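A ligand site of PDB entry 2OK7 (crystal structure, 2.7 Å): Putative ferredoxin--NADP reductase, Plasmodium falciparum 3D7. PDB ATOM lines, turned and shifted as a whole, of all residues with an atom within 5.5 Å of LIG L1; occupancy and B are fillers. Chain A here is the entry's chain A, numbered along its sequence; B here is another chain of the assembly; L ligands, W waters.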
ATOM      1  N   ASN A  33     -26.659 -19.397  -8.563  1.00  0.00           N
ATOM      2  CA  ASN A  33     -27.155 -19.534  -9.931  1.00  0.00           C
ATOM      3  C   ASN A  33     -28.117 -20.722 -10.022  1.00  0.00           C
ATOM      4  O   ASN A  33     -28.141 -21.562  -9.127  1.00  0.00           O
ATOM      5  CB  ASN A  33     -25.975 -19.685 -10.902  1.00  0.00           C
ATOM      6  CG  ASN A  33     -25.008 -18.493 -10.861  1.00  0.00           C
ATOM      7  OD1 ASN A  33     -25.420 -17.328 -10.875  1.00  0.00           O
ATOM      8  ND2 ASN A  33     -23.715 -18.781 -10.793  1.00  0.00           N
ATOM      9  N   LYS A 119     -28.848 -21.602 -18.073  1.00  0.00           N
ATOM     10  CA  LYS A 119     -28.940 -20.787 -16.869  1.00  0.00           C
ATOM     11  C   LYS A 119     -30.296 -20.073 -16.820  1.00  0.00           C
ATOM     12  O   LYS A 119     -30.714 -19.472 -17.806  1.00  0.00           O
ATOM     13  CB  LYS A 119     -27.777 -19.778 -16.840  1.00  0.00           C
ATOM     14  CG  LYS A 119     -27.851 -18.714 -15.754  1.00  0.00           C
ATOM     15  CD  LYS A 119     -26.556 -17.933 -15.638  1.00  0.00           C
ATOM     16  CE  LYS A 119     -26.678 -16.835 -14.604  1.00  0.00           C
ATOM     17  NZ  LYS A 119     -25.331 -16.348 -14.163  1.00  0.00           N
ATOM     18  N   THR A 178     -16.266 -18.893 -19.147  1.00  0.00           N
ATOM     19  CA  THR A 178     -16.977 -18.484 -17.943  1.00  0.00           C
ATOM     20  C   THR A 178     -18.409 -18.994 -17.997  1.00  0.00           C
ATOM     21  O   THR A 178     -19.026 -18.979 -19.060  1.00  0.00           O
ATOM     22  CB  THR A 178     -17.007 -16.949 -17.715  1.00  0.00           C
ATOM     23  OG1 THR A 178     -17.558 -16.291 -18.861  1.00  0.00           O
ATOM     24  CG2 THR A 178     -15.609 -16.402 -17.422  1.00  0.00           C
ATOM     25  N   GLY A 179     -18.905 -19.453 -16.853  1.00  0.00           N
ATOM     26  CA  GLY A 179     -20.309 -19.855 -16.675  1.00  0.00           C
ATOM     27  C   GLY A 179     -20.744 -20.996 -17.567  1.00  0.00           C
ATOM     28  O   GLY A 179     -20.179 -22.092 -17.543  1.00  0.00           O
ATOM     29  N   THR A 180     -21.744 -20.707 -18.399  1.00  0.00           N
ATOM     30  CA  THR A 180     -22.270 -21.667 -19.368  1.00  0.00           C
ATOM     31  C   THR A 180     -21.342 -21.874 -20.570  1.00  0.00           C
ATOM     32  O   THR A 180     -21.562 -22.770 -21.399  1.00  0.00           O
ATOM     33  CB  THR A 180     -23.691 -21.285 -19.815  1.00  0.00           C
ATOM     34  OG1 THR A 180     -23.702 -19.928 -20.305  1.00  0.00           O
ATOM     35  CG2 THR A 180     -24.697 -21.425 -18.664  1.00  0.00           C
ATOM     36  N   GLY A 216     -13.805 -19.704 -15.239  1.00  0.00           N
ATOM     37  CA  GLY A 216     -14.261 -18.792 -14.209  1.00  0.00           C
ATOM     38  C   GLY A 216     -15.723 -18.981 -13.881  1.00  0.00           C
ATOM     39  O   GLY A 216     -16.575 -18.801 -14.756  1.00  0.00           O
ATOM     40  N   VAL A 217     -16.011 -19.370 -12.642  1.00  0.00           N
ATOM     41  CA  VAL A 217     -17.362 -19.369 -12.097  1.00  0.00           C
ATOM     42  C   VAL A 217     -17.347 -18.718 -10.709  1.00  0.00           C
ATOM     43  O   VAL A 217     -16.297 -18.308 -10.232  1.00  0.00           O
ATOM     44  CB  VAL A 217     -17.959 -20.793 -12.017  1.00  0.00           C
ATOM     45  CG1 VAL A 217     -18.489 -21.235 -13.380  1.00  0.00           C
ATOM     46  CG2 VAL A 217     -16.950 -21.778 -11.461  1.00  0.00           C
ATOM     47  N   TYR A 218     -18.524 -18.604 -10.077  1.00  0.00           N
ATOM     48  CA  TYR A 218     -18.627 -17.985  -8.763  1.00  0.00           C
ATOM     49  C   TYR A 218     -17.831 -18.765  -7.721  1.00  0.00           C
ATOM     50  O   TYR A 218     -16.908 -18.226  -7.115  1.00  0.00           O
ATOM     51  CB  TYR A 218     -20.092 -17.888  -8.350  1.00  0.00           C
ATOM     52  CG  TYR A 218     -20.338 -17.059  -7.100  1.00  0.00           C
ATOM     53  CD1 TYR A 218     -20.303 -15.651  -7.144  1.00  0.00           C
ATOM     54  CD2 TYR A 218     -20.636 -17.670  -5.871  1.00  0.00           C
ATOM     55  CE1 TYR A 218     -20.545 -14.882  -5.999  1.00  0.00           C
ATOM     56  CE2 TYR A 218     -20.878 -16.900  -4.726  1.00  0.00           C
ATOM     57  CZ  TYR A 218     -20.828 -15.510  -4.805  1.00  0.00           C
ATOM     58  OH  TYR A 218     -21.077 -14.753  -3.688  1.00  0.00           O
ATOM     59  N   VAL A 245     -11.056 -20.453 -11.650  1.00  0.00           N
ATOM     60  CA  VAL A 245     -10.874 -19.092 -11.109  1.00  0.00           C
ATOM     61  C   VAL A 245     -12.178 -18.613 -10.473  1.00  0.00           C
ATOM     62  O   VAL A 245     -13.075 -18.130 -11.158  1.00  0.00           O
ATOM     63  CB  VAL A 245     -10.403 -18.083 -12.208  1.00  0.00           C
ATOM     64  CG1 VAL A 245     -10.045 -16.730 -11.599  1.00  0.00           C
ATOM     65  CG2 VAL A 245      -9.219 -18.641 -12.972  1.00  0.00           C
ATOM     66  N   SER A 247     -14.791 -16.351  -8.523  1.00  0.00           N
ATOM     67  CA  SER A 247     -14.987 -14.909  -8.305  1.00  0.00           C
ATOM     68  C   SER A 247     -15.389 -14.567  -6.872  1.00  0.00           C
ATOM     69  O   SER A 247     -15.269 -13.407  -6.462  1.00  0.00           O
ATOM     70  CB  SER A 247     -15.988 -14.305  -9.291  1.00  0.00           C
ATOM     71  OG  SER A 247     -17.322 -14.721  -9.048  1.00  0.00           O
ATOM     72  N   TYR A 258     -10.700 -11.944 -12.066  1.00  0.00           N
ATOM     73  CA  TYR A 258     -11.401 -12.822 -12.970  1.00  0.00           C
ATOM     74  C   TYR A 258     -10.417 -13.697 -13.740  1.00  0.00           C
ATOM     75  O   TYR A 258      -9.211 -13.620 -13.534  1.00  0.00           O
ATOM     76  CB  TYR A 258     -12.259 -11.982 -13.909  1.00  0.00           C
ATOM     77  CG  TYR A 258     -13.413 -11.295 -13.232  1.00  0.00           C
ATOM     78  CD1 TYR A 258     -13.497  -9.909 -13.186  1.00  0.00           C
ATOM     79  CD2 TYR A 258     -14.431 -12.024 -12.626  1.00  0.00           C
ATOM     80  CE1 TYR A 258     -14.563  -9.273 -12.562  1.00  0.00           C
ATOM     81  CE2 TYR A 258     -15.492 -11.399 -12.009  1.00  0.00           C
ATOM     82  CZ  TYR A 258     -15.558 -10.023 -11.977  1.00  0.00           C
ATOM     83  OH  TYR A 258     -16.610  -9.403 -11.359  1.00  0.00           O
ATOM     84  N   VAL A 259     -10.951 -14.523 -14.641  1.00  0.00           N
ATOM     85  CA  VAL A 259     -10.171 -15.495 -15.414  1.00  0.00           C
ATOM     86  C   VAL A 259      -9.021 -14.874 -16.268  1.00  0.00           C
ATOM     87  O   VAL A 259      -8.018 -15.537 -16.525  1.00  0.00           O
ATOM     88  CB  VAL A 259     -11.122 -16.426 -16.239  1.00  0.00           C
ATOM     89  CG1 VAL A 259     -11.551 -15.789 -17.565  1.00  0.00           C
ATOM     90  CG2 VAL A 259     -10.499 -17.784 -16.462  1.00  0.00           C
ATOM     91  N   GLN A 260      -9.161 -13.597 -16.639  1.00  0.00           N
ATOM     92  CA  GLN A 260      -8.161 -12.851 -17.422  1.00  0.00           C
ATOM     93  C   GLN A 260      -6.915 -12.621 -16.603  1.00  0.00           C
ATOM     94  O   GLN A 260      -5.796 -12.645 -17.132  1.00  0.00           O
ATOM     95  CB  GLN A 260      -8.663 -11.460 -17.797  1.00  0.00           C
ATOM     96  CG  GLN A 260      -9.868 -11.397 -18.671  1.00  0.00           C
ATOM     97  CD  GLN A 260     -11.101 -11.128 -17.881  1.00  0.00           C
ATOM     98  OE1 GLN A 260     -11.570  -9.996 -17.797  1.00  0.00           O
ATOM     99  NE2 GLN A 260     -11.651 -12.169 -17.285  1.00  0.00           N
ATOM    100  N   HIS A 286     -17.867 -14.250 -21.036  1.00  0.00           N
ATOM    101  CA  HIS A 286     -17.858 -12.794 -20.883  1.00  0.00           C
ATOM    102  C   HIS A 286     -16.975 -12.090 -21.930  1.00  0.00           C
ATOM    103  O   HIS A 286     -15.982 -12.643 -22.409  1.00  0.00           O
ATOM    104  CB  HIS A 286     -17.465 -12.388 -19.453  1.00  0.00           C
ATOM    105  CG  HIS A 286     -18.568 -12.547 -18.452  1.00  0.00           C
ATOM    106  ND1 HIS A 286     -19.499 -11.552 -18.200  1.00  0.00           N
ATOM    107  CD2 HIS A 286     -18.888 -13.571 -17.624  1.00  0.00           C
ATOM    108  CE1 HIS A 286     -20.340 -11.965 -17.278  1.00  0.00           C
ATOM    109  NE2 HIS A 286     -20.004 -13.181 -16.911  1.00  0.00           N
ATOM    110  N   SER A 288     -15.162  -9.440 -21.686  1.00  0.00           N
ATOM    111  CA  SER A 288     -13.919  -8.886 -21.143  1.00  0.00           C
ATOM    112  C   SER A 288     -12.711  -9.793 -21.333  1.00  0.00           C
ATOM    113  O   SER A 288     -11.576  -9.304 -21.321  1.00  0.00           O
ATOM    114  CB  SER A 288     -14.086  -8.595 -19.661  1.00  0.00           C
ATOM    115  OG  SER A 288     -15.305  -7.908 -19.409  1.00  0.00           O
ATOM    116  N   ILE A 289     -12.942 -11.093 -21.495  1.00  0.00           N
ATOM    117  CA  ILE A 289     -11.886 -12.086 -21.694  1.00  0.00           C
ATOM    118  C   ILE A 289     -11.082 -11.825 -22.974  1.00  0.00           C
ATOM    119  O   ILE A 289      -9.856 -11.971 -22.989  1.00  0.00           O
ATOM    120  CB  ILE A 289     -12.421 -13.529 -21.712  1.00  0.00           C
ATOM    121  CG1 ILE A 289     -13.398 -13.782 -20.557  1.00  0.00           C
ATOM    122  CG2 ILE A 289     -11.272 -14.523 -21.625  1.00  0.00           C
ATOM    123  CD1 ILE A 289     -14.203 -15.059 -20.684  1.00  0.00           C
ATOM    124  N   TYR B 258     -13.033  -2.604 -11.287  1.00  0.00           N
ATOM    125  CA  TYR B 258     -14.326  -2.099 -11.763  1.00  0.00           C
ATOM    126  C   TYR B 258     -14.988  -1.128 -10.789  1.00  0.00           C
ATOM    127  O   TYR B 258     -14.332  -0.614  -9.878  1.00  0.00           O
ATOM    128  CB  TYR B 258     -15.243  -3.265 -12.136  1.00  0.00           C
ATOM    129  CG  TYR B 258     -14.758  -4.074 -13.316  1.00  0.00           C
ATOM    130  CD1 TYR B 258     -14.548  -3.479 -14.562  1.00  0.00           C
ATOM    131  CD2 TYR B 258     -14.494  -5.455 -13.195  1.00  0.00           C
ATOM    132  CE1 TYR B 258     -14.097  -4.219 -15.645  1.00  0.00           C
ATOM    133  CE2 TYR B 258     -14.046  -6.201 -14.285  1.00  0.00           C
ATOM    134  CZ  TYR B 258     -13.850  -5.566 -15.503  1.00  0.00           C
ATOM    135  OH  TYR B 258     -13.409  -6.284 -16.587  1.00  0.00           O
ATOM    136  N   LYS B 287     -24.599  -7.524 -13.755  1.00  0.00           N
ATOM    137  CA  LYS B 287     -25.113  -8.152 -12.537  1.00  0.00           C
ATOM    138  C   LYS B 287     -24.112  -8.316 -11.390  1.00  0.00           C
ATOM    139  O   LYS B 287     -24.521  -8.435 -10.238  1.00  0.00           O
ATOM    140  CB  LYS B 287     -25.825  -9.481 -12.859  1.00  0.00           C
ATOM    141  CG  LYS B 287     -24.903 -10.659 -13.171  1.00  0.00           C
ATOM    142  CD  LYS B 287     -25.600 -11.985 -12.906  1.00  0.00           C
ATOM    143  CE  LYS B 287     -24.606 -13.152 -12.848  1.00  0.00           C
ATOM    144  NZ  LYS B 287     -23.726 -13.119 -11.637  1.00  0.00           N
ATOM    145  N   SER B 288     -22.819  -8.283 -11.712  1.00  0.00           N
ATOM    146  CA  SER B 288     -21.747  -8.433 -10.726  1.00  0.00           C
ATOM    147  C   SER B 288     -21.666  -7.302  -9.701  1.00  0.00           C
ATOM    148  O   SER B 288     -21.130  -7.499  -8.608  1.00  0.00           O
ATOM    149  CB  SER B 288     -20.393  -8.542 -11.432  1.00  0.00           C
ATOM    150  OG  SER B 288     -20.519  -9.218 -12.673  1.00  0.00           O
HETATM  151  P1  LIG L   1     -19.116 -12.345 -10.645  1.00  0.00           P
HETATM  152  O1  LIG L   1     -18.220 -11.247 -10.129  1.00  0.00           O
HETATM  153  O2  LIG L   1     -20.273 -11.887 -11.512  1.00  0.00           O
HETATM  154  O3  LIG L   1     -19.550 -13.375  -9.615  1.00  0.00           O
HETATM  155  P2  LIG L   1     -22.140 -15.334 -15.186  1.00  0.00           P
HETATM  156  O4  LIG L   1     -22.383 -16.293 -16.331  1.00  0.00           O
HETATM  157  O5  LIG L   1     -22.393 -13.888 -15.528  1.00  0.00           O
HETATM  158  O6  LIG L   1     -22.674 -15.787 -13.859  1.00  0.00           O
HETATM  159  O7  LIG L   1     -20.555 -15.339 -14.982  1.00  0.00           O
HETATM  160  C1  LIG L   1     -19.858 -16.475 -14.487  1.00  0.00           C
HETATM  161  C2  LIG L   1     -18.582 -15.978 -13.835  1.00  0.00           C
HETATM  162  O8  LIG L   1     -17.975 -14.995 -14.676  1.00  0.00           O
HETATM  163  C3  LIG L   1     -18.893 -15.299 -12.507  1.00  0.00           C
HETATM  164  O9  LIG L   1     -17.998 -15.762 -11.497  1.00  0.00           O
HETATM  165  C4  LIG L   1     -18.645 -13.834 -12.759  1.00  0.00           C
HETATM  166  O10 LIG L   1     -18.126 -13.160 -11.614  1.00  0.00           O
HETATM  167  C5  LIG L   1     -17.609 -13.881 -13.856  1.00  0.00           C
HETATM  168  N1  LIG L   1     -17.472 -12.559 -14.511  1.00  0.00           N
HETATM  169  C6  LIG L   1     -18.263 -11.480 -14.314  1.00  0.00           C
HETATM  170  N2  LIG L   1     -17.826 -10.425 -15.026  1.00  0.00           N
HETATM  171  C7  LIG L   1     -16.723 -10.815 -15.690  1.00  0.00           C
HETATM  172  C8  LIG L   1     -15.766 -10.175 -16.627  1.00  0.00           C
HETATM  173  N3  LIG L   1     -15.925  -8.888 -16.984  1.00  0.00           N
HETATM  174  N4  LIG L   1     -14.738 -10.911 -17.101  1.00  0.00           N
HETATM  175  C9  LIG L   1     -14.608 -12.206 -16.723  1.00  0.00           C
HETATM  176  N5  LIG L   1     -15.424 -12.845 -15.881  1.00  0.00           N
HETATM  177  C10 LIG L   1     -16.500 -12.212 -15.349  1.00  0.00           C
HETATM  178  P1  LG2 L   2     -14.084  -4.239 -19.635  1.00  0.00           P
HETATM  179  O1  LG2 L   2     -13.235  -5.075 -18.710  1.00  0.00           O
HETATM  180  O2  LG2 L   2     -15.083  -5.030 -20.449  1.00  0.00           O
HETATM  181  O3  LG2 L   2     -13.318  -3.215 -20.429  1.00  0.00           O
HETATM  182  P2  LG2 L   2     -19.898  -3.175 -21.561  1.00  0.00           P
HETATM  183  O4  LG2 L   2     -21.032  -4.158 -21.342  1.00  0.00           O
HETATM  184  O5  LG2 L   2     -18.590  -3.816 -21.966  1.00  0.00           O
HETATM  185  O6  LG2 L   2     -20.249  -1.978 -22.416  1.00  0.00           O
HETATM  186  O7  LG2 L   2     -19.608  -2.621 -20.073  1.00  0.00           O
HETATM  187  C1  LG2 L   2     -19.054  -1.333 -19.839  1.00  0.00           C
HETATM  188  C2  LG2 L   2     -17.986  -1.382 -18.770  1.00  0.00           C
HETATM  189  O8  LG2 L   2     -18.284  -2.400 -17.801  1.00  0.00           O
HETATM  190  C3  LG2 L   2     -16.634  -1.733 -19.372  1.00  0.00           C
HETATM  191  O9  LG2 L   2     -15.681  -0.837 -18.801  1.00  0.00           O
HETATM  192  C4  LG2 L   2     -16.338  -3.112 -18.839  1.00  0.00           C
HETATM  193  O10 LG2 L   2     -14.952  -3.346 -18.622  1.00  0.00           O
HETATM  194  C5  LG2 L   2     -17.078  -3.092 -17.514  1.00  0.00           C
HETATM  195  N1  LG2 L   2     -17.286  -4.448 -16.967  1.00  0.00           N
HETATM  196  C6  LG2 L   2     -17.070  -5.636 -17.579  1.00  0.00           C
HETATM  197  N2  LG2 L   2     -17.377  -6.658 -16.759  1.00  0.00           N
HETATM  198  C7  LG2 L   2     -17.762  -6.141 -15.577  1.00  0.00           C
HETATM  199  C8  LG2 L   2     -18.201  -6.671 -14.268  1.00  0.00           C
HETATM  200  N3  LG2 L   2     -18.290  -7.999 -14.057  1.00  0.00           N
HETATM  201  N4  LG2 L   2     -18.534  -5.788 -13.298  1.00  0.00           N
HETATM  202  C9  LG2 L   2     -18.453  -4.456 -13.523  1.00  0.00           C
HETATM  203  N5  LG2 L   2     -18.045  -3.907 -14.663  1.00  0.00           N
HETATM  204  C10 LG2 L   2     -17.697  -4.686 -15.720  1.00  0.00           C
HETATM  205  O   HOH W   1     -23.502 -15.019 -19.104  1.00  0.00           O
HETATM  206  O   HOH W   2     -17.096 -10.231  -7.752  1.00  0.00           O
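Residues that only touch LIG L1: Thr 178 (3.7 Å), Gly 179 (3.9 Å), Gly 216 (3.6 Å) and Tyr 258 of chain B (3.6 Å). 14 residues have an atom within 4 Å of LIG L1: Lys 119, Thr 178, Gly 179, Gly 216, Val 217, Tyr 218, Ser 247, Tyr 258 of chain A, Gln 260, His 286, Ser 288 of chain A, Tyr 258 of chain B, Lys 287 of chain B and Ser 288 of chain B. The nearest printed residue that does not touch LIG L1 is Ile 289 (4.3 Å).
A nitrogen (N2) of LIG L1 sits at hydrogen-bond distance from a nitrogen (N3) of LG2 L2, 2.7 Å away.
O5 of LIG L1 sits at hydrogen-bond distance from NE2 of His 286. An oxygen (O6) of LIG L1 lies within salt-bridge range of the side-chain amino group (NZ) of Lys 119, at 2.7 Å. The side-chain hydroxyl of Tyr 258 of chain A lies within hydrogen-bond range of an oxygen (O1) of LIG L1 (2.7 Å). O6 of LIG L1 is in salt-bridge range of NZ of Lys 287 of chain B. A nitrogen (N3) of LIG L1 sits at hydrogen-bond distance from the side-chain hydroxyl (OG) of Ser 288 of chain A (2.7 Å). The backbone NH of Tyr 218 lies within hydrogen-bond range of an oxygen (O9) of LIG L1, at 3.2 Å. An oxygen (O3) of LIG L1 lies within hydrogen-bond range of the side-chain hydroxyl (OG) of Ser 247 (2.7 Å). A nitrogen (N4) of LIG L1 sits close to the side-chain amide nitrogen of Gln 260, 3.3 Å away. O1 of LG2 L2 lies within hydrogen-bond range of OH of Tyr 258 of chain B, at 2.4 Å. OG of Ser 288 of chain A lies within hydrogen-bond range of O2 of LG2 L2, at 3.1 Å. O2 of LIG L1 is in hydrogen-bond range of OG of Ser 288 of chain B (2.9 Å). OG of Ser 288 of chain B sits at hydrogen-bond distance from N3 of LG2 L2 (2.9 Å). OH of Tyr 258 of chain A sits at hydrogen-bond distance from N3 of LG2 L2, 3.5 Å away. O of Val 217 lies close to O9 of LIG L1, at 3.3 Å.
The side-chain hydroxyl of Thr 178 is in hydrogen-bond range of the backbone NH of His 286, at 3.0 Å. The backbone NH of Ser 247 is in hydrogen-bond range of the backbone carbonyl oxygen of Val 217 (3.0 Å). The backbone carbonyl oxygen (O) of Gly 216 lies within hydrogen-bond range of the backbone NH (N) of Gly 179, at 3.2 Å. The side-chain amino group (NZ) of Lys 119 lies within hydrogen-bond range of the side-chain amide oxygen (OD1) of Asn 33, at 3.4 Å. N of Ser 247 sits at hydrogen-bond distance from O of Tyr 218, 3.2 Å away.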
